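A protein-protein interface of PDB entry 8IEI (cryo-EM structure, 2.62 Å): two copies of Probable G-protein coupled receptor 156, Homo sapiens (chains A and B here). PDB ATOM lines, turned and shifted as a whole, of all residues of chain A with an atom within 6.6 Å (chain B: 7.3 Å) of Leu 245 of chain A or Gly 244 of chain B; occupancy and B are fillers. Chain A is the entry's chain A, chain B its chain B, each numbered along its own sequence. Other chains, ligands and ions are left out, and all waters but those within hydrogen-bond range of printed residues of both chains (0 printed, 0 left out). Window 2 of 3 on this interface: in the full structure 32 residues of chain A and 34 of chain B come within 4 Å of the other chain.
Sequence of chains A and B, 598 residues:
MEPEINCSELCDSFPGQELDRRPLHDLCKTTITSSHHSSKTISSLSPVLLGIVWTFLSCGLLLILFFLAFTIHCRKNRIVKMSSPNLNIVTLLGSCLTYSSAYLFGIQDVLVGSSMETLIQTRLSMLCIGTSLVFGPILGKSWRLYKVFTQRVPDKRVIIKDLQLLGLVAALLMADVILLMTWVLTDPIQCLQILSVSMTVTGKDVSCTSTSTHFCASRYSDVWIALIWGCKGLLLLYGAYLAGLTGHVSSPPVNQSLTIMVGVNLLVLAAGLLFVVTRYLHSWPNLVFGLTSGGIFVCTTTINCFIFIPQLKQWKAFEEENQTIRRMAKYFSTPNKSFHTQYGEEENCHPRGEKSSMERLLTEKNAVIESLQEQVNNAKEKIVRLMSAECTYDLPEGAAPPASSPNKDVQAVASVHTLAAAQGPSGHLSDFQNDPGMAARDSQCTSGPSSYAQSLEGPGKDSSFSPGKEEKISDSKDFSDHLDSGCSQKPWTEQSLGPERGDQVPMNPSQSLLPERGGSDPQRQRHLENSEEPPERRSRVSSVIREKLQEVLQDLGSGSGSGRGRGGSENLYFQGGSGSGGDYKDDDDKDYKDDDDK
OG of Ser 257 of chain A is in hydrogen-bond range of O of Ala 243 of chain A.
O of Ala 243 of chain B sits at hydrogen-bond distance from OG of Ser 257 of chain B (2.6 Å).
Of the 14 printed residues of chain A, 6 touch a printed residue of chain B.
Hydrophobic or aromatic side chains of chain A within 4 Å of the printed part of chain B: Tyr 146, Tyr 241 and Leu 245.
Along chain A the printed residues that touch a printed residue of chain B span positions 146 to 245.
Of the 15 printed residues of chain B, 7 touch a printed residue of chain A.
Printed residues of chain B that touch a printed residue of chain A: Ala 240, Tyr 241, Ala 243, Gly 244, Leu 245, His 248 and Met 261.
Hydrophobic or aromatic side chains of chain B that line the printed part of chain A: Tyr 241, Leu 245, His 248 and Met 261.
Among the printed residues, no Asp or Glu carboxylate lies within 4 Å of a Lys or Arg side-chain nitrogen of the other chain.
Tyr 241 of chain B touches Ala 240 of chain A (CA to O, 3.6 Å).
CA of Tyr 241 of chain A touches O of Ala 240 of chain B, at 3.6 Å.
CE1 of Tyr 241 of chain A touches O of Ala 243 of chain B, at 3.9 Å.
Tyr 241 of chain A touches Gly 244 of chain B (CD1 to N, 3.5 Å).
Met 261 of chain B touches Tyr 241 of chain A (CE to CB, 3.5 Å).
Ala 243 of chain A touches Tyr 241 of chain B.
N of Gly 244 of chain A touches CD1 of Tyr 241 of chain B, 3.5 Å away.
A ring nitrogen (NE2) of His 248 of chain B sits at hydrogen-bond distance from the side-chain hydroxyl of Tyr 146 of chain A.
O of Gly 244 of chain A lies close to N of Leu 245 of chain B, 3.5 Å away.
O of Gly 244 of chain B sits close to N of Leu 245 of chain A.
O of Gly 244 of chain A lies close to O of Gly 244 of chain B (3.5 Å).
Ala 240 of chain A touches Tyr 241 of chain B, and with the chains exchanged Tyr 241 of chain A touches Ala 240 of chain B.
Tyr 241 of chain A touches Ala 243 of chain B, and with the chains exchanged Ala 243 of chain A touches Tyr 241 of chain B.
Gly 244 of chain B touches its own counterpart, Gly 244 of chain A.
Gly 244 of chain A touches Leu 245 of chain B, and with the chains exchanged Leu 245 of chain A touches Gly 244 of chain B.
Positions printed for both chains: 238, 240, 241, 242, 243, 244, 245, 246, 247, 248, 249 and 257.
Of the 11 pairs that touch across the chains among the printed residues, 9 have their exchanged pair printed and touching as well.
Of chain A, only Tyr 241, Gly 244 and Leu 245 come within 4 Å of Gly 244 of chain B.
Of chain B, only Tyr 241, Gly 244 and Leu 245 come within 4 Å of Gly 244 of chain A.
Printed residues of chain A within 4 Å of Ala 240 of chain B: Tyr 241.
Of the printed residues of chain A, His 248 of chain B touches Tyr 146 (3.1 Å).
Of the printed residues of chain B, Tyr 146 of chain A touches His 248.
Of the printed residues of chain A, Leu 245 of chain B touches Gly 244.
Of the printed residues of chain A, Met 261 of chain B touches Tyr 241.
Thr 246 of chain B touches none of the printed residues of chain A.
Gly 239 of chain B touches none of the printed residues of chain A.
The nearest residue of chain B that does not touch Leu 245 of chain A is Leu 245 of chain B (4.1 Å).
The nearest residue of chain A that does not touch Gly 244 of chain B is Ala 240 of chain A (5.3 Å).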
ATOM      1  N   TYR A 146      -3.399  25.504  -6.166  1.00  0.00           N
ATOM      2  CA  TYR A 146      -2.208  24.749  -6.539  1.00  0.00           C
ATOM      3  C   TYR A 146      -2.539  23.632  -7.522  1.00  0.00           C
ATOM      4  O   TYR A 146      -1.829  23.443  -8.516  1.00  0.00           O
ATOM      5  CB  TYR A 146      -1.549  24.171  -5.288  1.00  0.00           C
ATOM      6  CG  TYR A 146      -0.458  23.172  -5.581  1.00  0.00           C
ATOM      7  CD1 TYR A 146       0.734  23.571  -6.165  1.00  0.00           C
ATOM      8  CD2 TYR A 146      -0.624  21.830  -5.280  1.00  0.00           C
ATOM      9  CE1 TYR A 146       1.731  22.662  -6.436  1.00  0.00           C
ATOM     10  CE2 TYR A 146       0.367  20.914  -5.548  1.00  0.00           C
ATOM     11  CZ  TYR A 146       1.542  21.334  -6.127  1.00  0.00           C
ATOM     12  OH  TYR A 146       2.533  20.420  -6.394  1.00  0.00           O
ATOM     13  N   PHE A 149      -3.348  25.004 -10.950  1.00  0.00           N
ATOM     14  CA  PHE A 149      -2.128  25.462 -11.608  1.00  0.00           C
ATOM     15  C   PHE A 149      -1.285  24.307 -12.134  1.00  0.00           C
ATOM     16  O   PHE A 149      -0.549  24.480 -13.110  1.00  0.00           O
ATOM     17  CB  PHE A 149      -1.304  26.305 -10.637  1.00  0.00           C
ATOM     18  CG  PHE A 149      -0.133  26.996 -11.273  1.00  0.00           C
ATOM     19  CD1 PHE A 149      -0.321  28.071 -12.123  1.00  0.00           C
ATOM     20  CD2 PHE A 149       1.159  26.579 -11.006  1.00  0.00           C
ATOM     21  CE1 PHE A 149       0.755  28.712 -12.703  1.00  0.00           C
ATOM     22  CE2 PHE A 149       2.239  27.217 -11.583  1.00  0.00           C
ATOM     23  CZ  PHE A 149       2.035  28.285 -12.433  1.00  0.00           C
ATOM     24  N   TYR A 238       1.862  22.706   7.210  1.00  0.00           N
ATOM     25  CA  TYR A 238       1.392  22.376   5.870  1.00  0.00           C
ATOM     26  C   TYR A 238       0.725  23.572   5.200  1.00  0.00           C
ATOM     27  O   TYR A 238       0.822  23.728   3.980  1.00  0.00           O
ATOM     28  CB  TYR A 238       0.430  21.191   5.904  1.00  0.00           C
ATOM     29  CG  TYR A 238       0.011  20.737   4.524  1.00  0.00           C
ATOM     30  CD1 TYR A 238       0.956  20.358   3.580  1.00  0.00           C
ATOM     31  CD2 TYR A 238      -1.325  20.702   4.157  1.00  0.00           C
ATOM     32  CE1 TYR A 238       0.584  19.953   2.319  1.00  0.00           C
ATOM     33  CE2 TYR A 238      -1.708  20.295   2.895  1.00  0.00           C
ATOM     34  CZ  TYR A 238      -0.748  19.922   1.981  1.00  0.00           C
ATOM     35  OH  TYR A 238      -1.118  19.515   0.722  1.00  0.00           O
ATOM     36  N   ALA A 240       1.601  26.752   5.631  1.00  0.00           N
ATOM     37  CA  ALA A 240       2.706  27.584   5.165  1.00  0.00           C
ATOM     38  C   ALA A 240       3.343  26.994   3.916  1.00  0.00           C
ATOM     39  O   ALA A 240       3.711  27.729   2.991  1.00  0.00           O
ATOM     40  CB  ALA A 240       3.745  27.740   6.274  1.00  0.00           C
ATOM     41  N   TYR A 241       3.478  25.668   3.871  1.00  0.00           N
ATOM     42  CA  TYR A 241       3.962  25.014   2.659  1.00  0.00           C
ATOM     43  C   TYR A 241       3.050  25.307   1.473  1.00  0.00           C
ATOM     44  O   TYR A 241       3.525  25.632   0.380  1.00  0.00           O
ATOM     45  CB  TYR A 241       4.065  23.509   2.904  1.00  0.00           C
ATOM     46  CG  TYR A 241       4.629  22.715   1.750  1.00  0.00           C
ATOM     47  CD1 TYR A 241       5.932  22.906   1.319  1.00  0.00           C
ATOM     48  CD2 TYR A 241       3.859  21.762   1.103  1.00  0.00           C
ATOM     49  CE1 TYR A 241       6.449  22.177   0.270  1.00  0.00           C
ATOM     50  CE2 TYR A 241       4.368  21.030   0.055  1.00  0.00           C
ATOM     51  CZ  TYR A 241       5.664  21.241  -0.357  1.00  0.00           C
ATOM     52  OH  TYR A 241       6.174  20.512  -1.402  1.00  0.00           O
ATOM     53  N   LEU A 242       1.736  25.206   1.676  1.00  0.00           N
ATOM     54  CA  LEU A 242       0.787  25.469   0.597  1.00  0.00           C
ATOM     55  C   LEU A 242       0.815  26.932   0.174  1.00  0.00           C
ATOM     56  O   LEU A 242       0.704  27.243  -1.016  1.00  0.00           O
ATOM     57  CB  LEU A 242      -0.623  25.073   1.028  1.00  0.00           C
ATOM     58  CG  LEU A 242      -1.081  23.654   0.695  1.00  0.00           C
ATOM     59  CD1 LEU A 242      -2.394  23.368   1.393  1.00  0.00           C
ATOM     60  CD2 LEU A 242      -1.217  23.456  -0.806  1.00  0.00           C
ATOM     61  N   ALA A 243       0.939  27.847   1.137  1.00  0.00           N
ATOM     62  CA  ALA A 243       1.038  29.264   0.811  1.00  0.00           C
ATOM     63  C   ALA A 243       2.283  29.548  -0.014  1.00  0.00           C
ATOM     64  O   ALA A 243       2.241  30.346  -0.956  1.00  0.00           O
ATOM     65  CB  ALA A 243       1.046  30.098   2.090  1.00  0.00           C
ATOM     66  N   GLY A 244       3.403  28.913   0.332  1.00  0.00           N
ATOM     67  CA  GLY A 244       4.594  29.047  -0.487  1.00  0.00           C
ATOM     68  C   GLY A 244       4.413  28.464  -1.874  1.00  0.00           C
ATOM     69  O   GLY A 244       4.891  29.030  -2.861  1.00  0.00           O
ATOM     70  N   LEU A 245       3.724  27.325  -1.972  1.00  0.00           N
ATOM     71  CA  LEU A 245       3.517  26.700  -3.273  1.00  0.00           C
ATOM     72  C   LEU A 245       2.715  27.605  -4.197  1.00  0.00           C
ATOM     73  O   LEU A 245       3.044  27.745  -5.380  1.00  0.00           O
ATOM     74  CB  LEU A 245       2.808  25.356  -3.108  1.00  0.00           C
ATOM     75  CG  LEU A 245       3.672  24.122  -2.836  1.00  0.00           C
ATOM     76  CD1 LEU A 245       2.779  22.939  -2.514  1.00  0.00           C
ATOM     77  CD2 LEU A 245       4.584  23.796  -4.008  1.00  0.00           C
ATOM     78  N   THR A 246       1.658  28.222  -3.678  1.00  0.00           N
ATOM     79  CA  THR A 246       0.860  29.182  -4.438  1.00  0.00           C
ATOM     80  C   THR A 246       1.362  30.604  -4.218  1.00  0.00           C
ATOM     81  O   THR A 246       0.598  31.509  -3.902  1.00  0.00           O
ATOM     82  CB  THR A 246      -0.608  29.062  -4.047  1.00  0.00           C
ATOM     83  OG1 THR A 246      -0.731  29.136  -2.622  1.00  0.00           O
ATOM     84  CG2 THR A 246      -1.175  27.744  -4.519  1.00  0.00           C
ATOM     85  N   GLY A 247       2.663  30.811  -4.395  1.00  0.00           N
ATOM     86  CA  GLY A 247       3.283  32.108  -4.201  1.00  0.00           C
ATOM     87  C   GLY A 247       3.355  32.860  -5.521  1.00  0.00           C
ATOM     88  O   GLY A 247       3.976  32.393  -6.478  1.00  0.00           O
ATOM     89  N   HIS A 248       2.714  34.026  -5.552  1.00  0.00           N
ATOM     90  CA  HIS A 248       2.663  34.849  -6.757  1.00  0.00           C
ATOM     91  C   HIS A 248       2.034  34.081  -7.917  1.00  0.00           C
ATOM     92  O   HIS A 248       2.486  34.161  -9.061  1.00  0.00           O
ATOM     93  CB  HIS A 248       4.060  35.348  -7.133  1.00  0.00           C
ATOM     94  CG  HIS A 248       4.847  35.873  -5.975  1.00  0.00           C
ATOM     95  ND1 HIS A 248       4.366  36.844  -5.124  1.00  0.00           N
ATOM     96  CD2 HIS A 248       6.082  35.554  -5.519  1.00  0.00           C
ATOM     97  CE1 HIS A 248       5.270  37.105  -4.198  1.00  0.00           C
ATOM     98  NE2 HIS A 248       6.321  36.334  -4.415  1.00  0.00           N
ATOM     99  N   VAL A 249       0.982  33.325  -7.618  1.00  0.00           N
ATOM    100  CA  VAL A 249       0.277  32.535  -8.619  1.00  0.00           C
ATOM    101  C   VAL A 249      -0.939  33.275  -9.165  1.00  0.00           C
ATOM    102  O   VAL A 249      -1.356  33.027 -10.295  1.00  0.00           O
ATOM    103  CB  VAL A 249      -0.116  31.160  -8.032  1.00  0.00           C
ATOM    104  CG1 VAL A 249      -1.182  30.467  -8.885  1.00  0.00           C
ATOM    105  CG2 VAL A 249       1.113  30.276  -7.915  1.00  0.00           C
ATOM    106  N   SER A 257      -2.293  33.644   0.140  1.00  0.00           N
ATOM    107  CA  SER A 257      -0.935  33.301   0.549  1.00  0.00           C
ATOM    108  C   SER A 257      -0.368  34.261   1.579  1.00  0.00           C
ATOM    109  O   SER A 257       0.325  33.828   2.501  1.00  0.00           O
ATOM    110  CB  SER A 257      -0.016  33.269  -0.679  1.00  0.00           C
ATOM    111  OG  SER A 257       1.320  32.987  -0.314  1.00  0.00           O
ATOM    112  N   TYR B 238       8.572  29.954   8.566  1.00  0.00           N
ATOM    113  CA  TYR B 238       9.190  30.590   7.407  1.00  0.00           C
ATOM    114  C   TYR B 238       9.969  29.583   6.567  1.00  0.00           C
ATOM    115  O   TYR B 238      10.026  29.713   5.341  1.00  0.00           O
ATOM    116  CB  TYR B 238      10.108  31.734   7.834  1.00  0.00           C
ATOM    117  CG  TYR B 238      10.639  32.525   6.660  1.00  0.00           C
ATOM    118  CD1 TYR B 238       9.779  33.182   5.791  1.00  0.00           C
ATOM    119  CD2 TYR B 238      12.001  32.601   6.409  1.00  0.00           C
ATOM    120  CE1 TYR B 238      10.257  33.895   4.716  1.00  0.00           C
ATOM    121  CE2 TYR B 238      12.489  33.315   5.336  1.00  0.00           C
ATOM    122  CZ  TYR B 238      11.612  33.960   4.492  1.00  0.00           C
ATOM    123  OH  TYR B 238      12.090  34.673   3.419  1.00  0.00           O
ATOM    124  N   GLY B 239      10.571  28.579   7.203  1.00  0.00           N
ATOM    125  CA  GLY B 239      11.247  27.537   6.448  1.00  0.00           C
ATOM    126  C   GLY B 239      10.295  26.712   5.605  1.00  0.00           C
ATOM    127  O   GLY B 239      10.617  26.340   4.477  1.00  0.00           O
ATOM    128  N   ALA B 240       9.117  26.402   6.144  1.00  0.00           N
ATOM    129  CA  ALA B 240       8.098  25.706   5.362  1.00  0.00           C
ATOM    130  C   ALA B 240       7.611  26.571   4.209  1.00  0.00           C
ATOM    131  O   ALA B 240       7.358  26.068   3.107  1.00  0.00           O
ATOM    132  CB  ALA B 240       6.932  25.302   6.260  1.00  0.00           C
ATOM    133  N   TYR B 241       7.471  27.876   4.445  1.00  0.00           N
ATOM    134  CA  TYR B 241       7.124  28.792   3.364  1.00  0.00           C
ATOM    135  C   TYR B 241       8.184  28.779   2.267  1.00  0.00           C
ATOM    136  O   TYR B 241       7.856  28.751   1.077  1.00  0.00           O
ATOM    137  CB  TYR B 241       6.944  30.203   3.923  1.00  0.00           C
ATOM    138  CG  TYR B 241       6.481  31.226   2.913  1.00  0.00           C
ATOM    139  CD1 TYR B 241       5.257  31.096   2.275  1.00  0.00           C
ATOM    140  CD2 TYR B 241       7.264  32.326   2.603  1.00  0.00           C
ATOM    141  CE1 TYR B 241       4.829  32.029   1.359  1.00  0.00           C
ATOM    142  CE2 TYR B 241       6.846  33.262   1.687  1.00  0.00           C
ATOM    143  CZ  TYR B 241       5.628  33.109   1.067  1.00  0.00           C
ATOM    144  OH  TYR B 241       5.202  34.041   0.150  1.00  0.00           O
ATOM    145  N   LEU B 242       9.462  28.801   2.653  1.00  0.00           N
ATOM    146  CA  LEU B 242      10.543  28.752   1.672  1.00  0.00           C
ATOM    147  C   LEU B 242      10.561  27.425   0.925  1.00  0.00           C
ATOM    148  O   LEU B 242      10.828  27.387  -0.281  1.00  0.00           O
ATOM    149  CB  LEU B 242      11.888  28.981   2.360  1.00  0.00           C
ATOM    150  CG  LEU B 242      12.366  30.421   2.534  1.00  0.00           C
ATOM    151  CD1 LEU B 242      13.640  30.436   3.355  1.00  0.00           C
ATOM    152  CD2 LEU B 242      12.591  31.097   1.191  1.00  0.00           C
ATOM    153  N   ALA B 243      10.306  26.322   1.628  1.00  0.00           N
ATOM    154  CA  ALA B 243      10.247  25.021   0.975  1.00  0.00           C
ATOM    155  C   ALA B 243       9.120  24.973  -0.044  1.00  0.00           C
ATOM    156  O   ALA B 243       9.280  24.405  -1.129  1.00  0.00           O
ATOM    157  CB  ALA B 243      10.074  23.919   2.018  1.00  0.00           C
ATOM    158  N   GLY B 244       7.966  25.549   0.292  1.00  0.00           N
ATOM    159  CA  GLY B 244       6.879  25.615  -0.669  1.00  0.00           C
ATOM    160  C   GLY B 244       7.197  26.511  -1.850  1.00  0.00           C
ATOM    161  O   GLY B 244       6.870  26.185  -2.994  1.00  0.00           O
ATOM    162  N   LEU B 245       7.835  27.655  -1.592  1.00  0.00           N
ATOM    163  CA  LEU B 245       8.180  28.582  -2.662  1.00  0.00           C
ATOM    164  C   LEU B 245       9.137  27.970  -3.671  1.00  0.00           C
ATOM    165  O   LEU B 245       9.123  28.369  -4.840  1.00  0.00           O
ATOM    166  CB  LEU B 245       8.813  29.850  -2.085  1.00  0.00           C
ATOM    167  CG  LEU B 245       7.893  31.027  -1.765  1.00  0.00           C
ATOM    168  CD1 LEU B 245       8.668  32.075  -0.996  1.00  0.00           C
ATOM    169  CD2 LEU B 245       7.283  31.625  -3.022  1.00  0.00           C
ATOM    170  N   THR B 246       9.962  27.017  -3.245  1.00  0.00           N
ATOM    171  CA  THR B 246      10.962  26.399  -4.102  1.00  0.00           C
ATOM    172  C   THR B 246      10.593  24.935  -4.307  1.00  0.00           C
ATOM    173  O   THR B 246      11.466  24.066  -4.365  1.00  0.00           O
ATOM    174  CB  THR B 246      12.351  26.540  -3.470  1.00  0.00           C
ATOM    175  OG1 THR B 246      12.504  27.863  -2.945  1.00  0.00           O
ATOM    176  CG2 THR B 246      13.438  26.325  -4.496  1.00  0.00           C
ATOM    177  N   GLY B 247       9.296  24.663  -4.420  1.00  0.00           N
ATOM    178  CA  GLY B 247       8.783  23.307  -4.407  1.00  0.00           C
ATOM    179  C   GLY B 247       9.276  22.423  -5.533  1.00  0.00           C
ATOM    180  O   GLY B 247       9.674  21.279  -5.298  1.00  0.00           O
ATOM    181  N   HIS B 248       9.247  22.937  -6.759  1.00  0.00           N
ATOM    182  CA  HIS B 248       9.634  22.195  -7.955  1.00  0.00           C
ATOM    183  C   HIS B 248      10.549  23.043  -8.825  1.00  0.00           C
ATOM    184  O   HIS B 248      10.357  23.172 -10.036  1.00  0.00           O
ATOM    185  CB  HIS B 248       8.401  21.752  -8.737  1.00  0.00           C
ATOM    186  CG  HIS B 248       7.380  21.041  -7.903  1.00  0.00           C
ATOM    187  ND1 HIS B 248       7.545  19.742  -7.472  1.00  0.00           N
ATOM    188  CD2 HIS B 248       6.183  21.450  -7.418  1.00  0.00           C
ATOM    189  CE1 HIS B 248       6.493  19.381  -6.760  1.00  0.00           C
ATOM    190  NE2 HIS B 248       5.652  20.398  -6.711  1.00  0.00           N
ATOM    191  N   VAL B 249      11.568  23.636  -8.206  1.00  0.00           N
ATOM    192  CA  VAL B 249      12.455  24.575  -8.883  1.00  0.00           C
ATOM    193  C   VAL B 249      13.739  23.882  -9.327  1.00  0.00           C
ATOM    194  O   VAL B 249      14.427  24.359 -10.236  1.00  0.00           O
ATOM    195  CB  VAL B 249      12.763  25.780  -7.973  1.00  0.00           C
ATOM    196  CG1 VAL B 249      13.847  26.662  -8.572  1.00  0.00           C
ATOM    197  CG2 VAL B 249      11.501  26.591  -7.737  1.00  0.00           C
ATOM    198  N   SER B 257      13.276  21.129  -0.432  1.00  0.00           N
ATOM    199  CA  SER B 257      11.927  21.253   0.114  1.00  0.00           C
ATOM    200  C   SER B 257      11.524  20.012   0.904  1.00  0.00           C
ATOM    201  O   SER B 257      10.934  20.125   1.986  1.00  0.00           O
ATOM    202  CB  SER B 257      10.936  21.516  -1.016  1.00  0.00           C
ATOM    203  OG  SER B 257      11.205  22.760  -1.630  1.00  0.00           O
ATOM    204  N   ILE B 260      13.316  19.868   4.240  1.00  0.00           N
ATOM    205  CA  ILE B 260      12.765  20.855   5.165  1.00  0.00           C
ATOM    206  C   ILE B 260      11.444  20.363   5.742  1.00  0.00           C
ATOM    207  O   ILE B 260      11.204  20.464   6.949  1.00  0.00           O
ATOM    208  CB  ILE B 260      12.598  22.218   4.467  1.00  0.00           C
ATOM    209  CG1 ILE B 260      13.955  22.913   4.346  1.00  0.00           C
ATOM    210  CG2 ILE B 260      11.614  23.114   5.239  1.00  0.00           C
ATOM    211  CD1 ILE B 260      13.972  24.087   3.391  1.00  0.00           C
ATOM    212  N   MET B 261      10.560  19.840   4.891  1.00  0.00           N
ATOM    213  CA  MET B 261       9.243  19.440   5.377  1.00  0.00           C
ATOM    214  C   MET B 261       9.342  18.250   6.324  1.00  0.00           C
ATOM    215  O   MET B 261       8.724  18.249   7.400  1.00  0.00           O
ATOM    216  CB  MET B 261       8.326  19.114   4.197  1.00  0.00           C
ATOM    217  CG  MET B 261       7.716  20.320   3.472  1.00  0.00           C
ATOM    218  SD  MET B 261       7.010  21.623   4.507  1.00  0.00           S
ATOM    219  CE  MET B 261       5.394  20.939   4.859  1.00  0.00           C
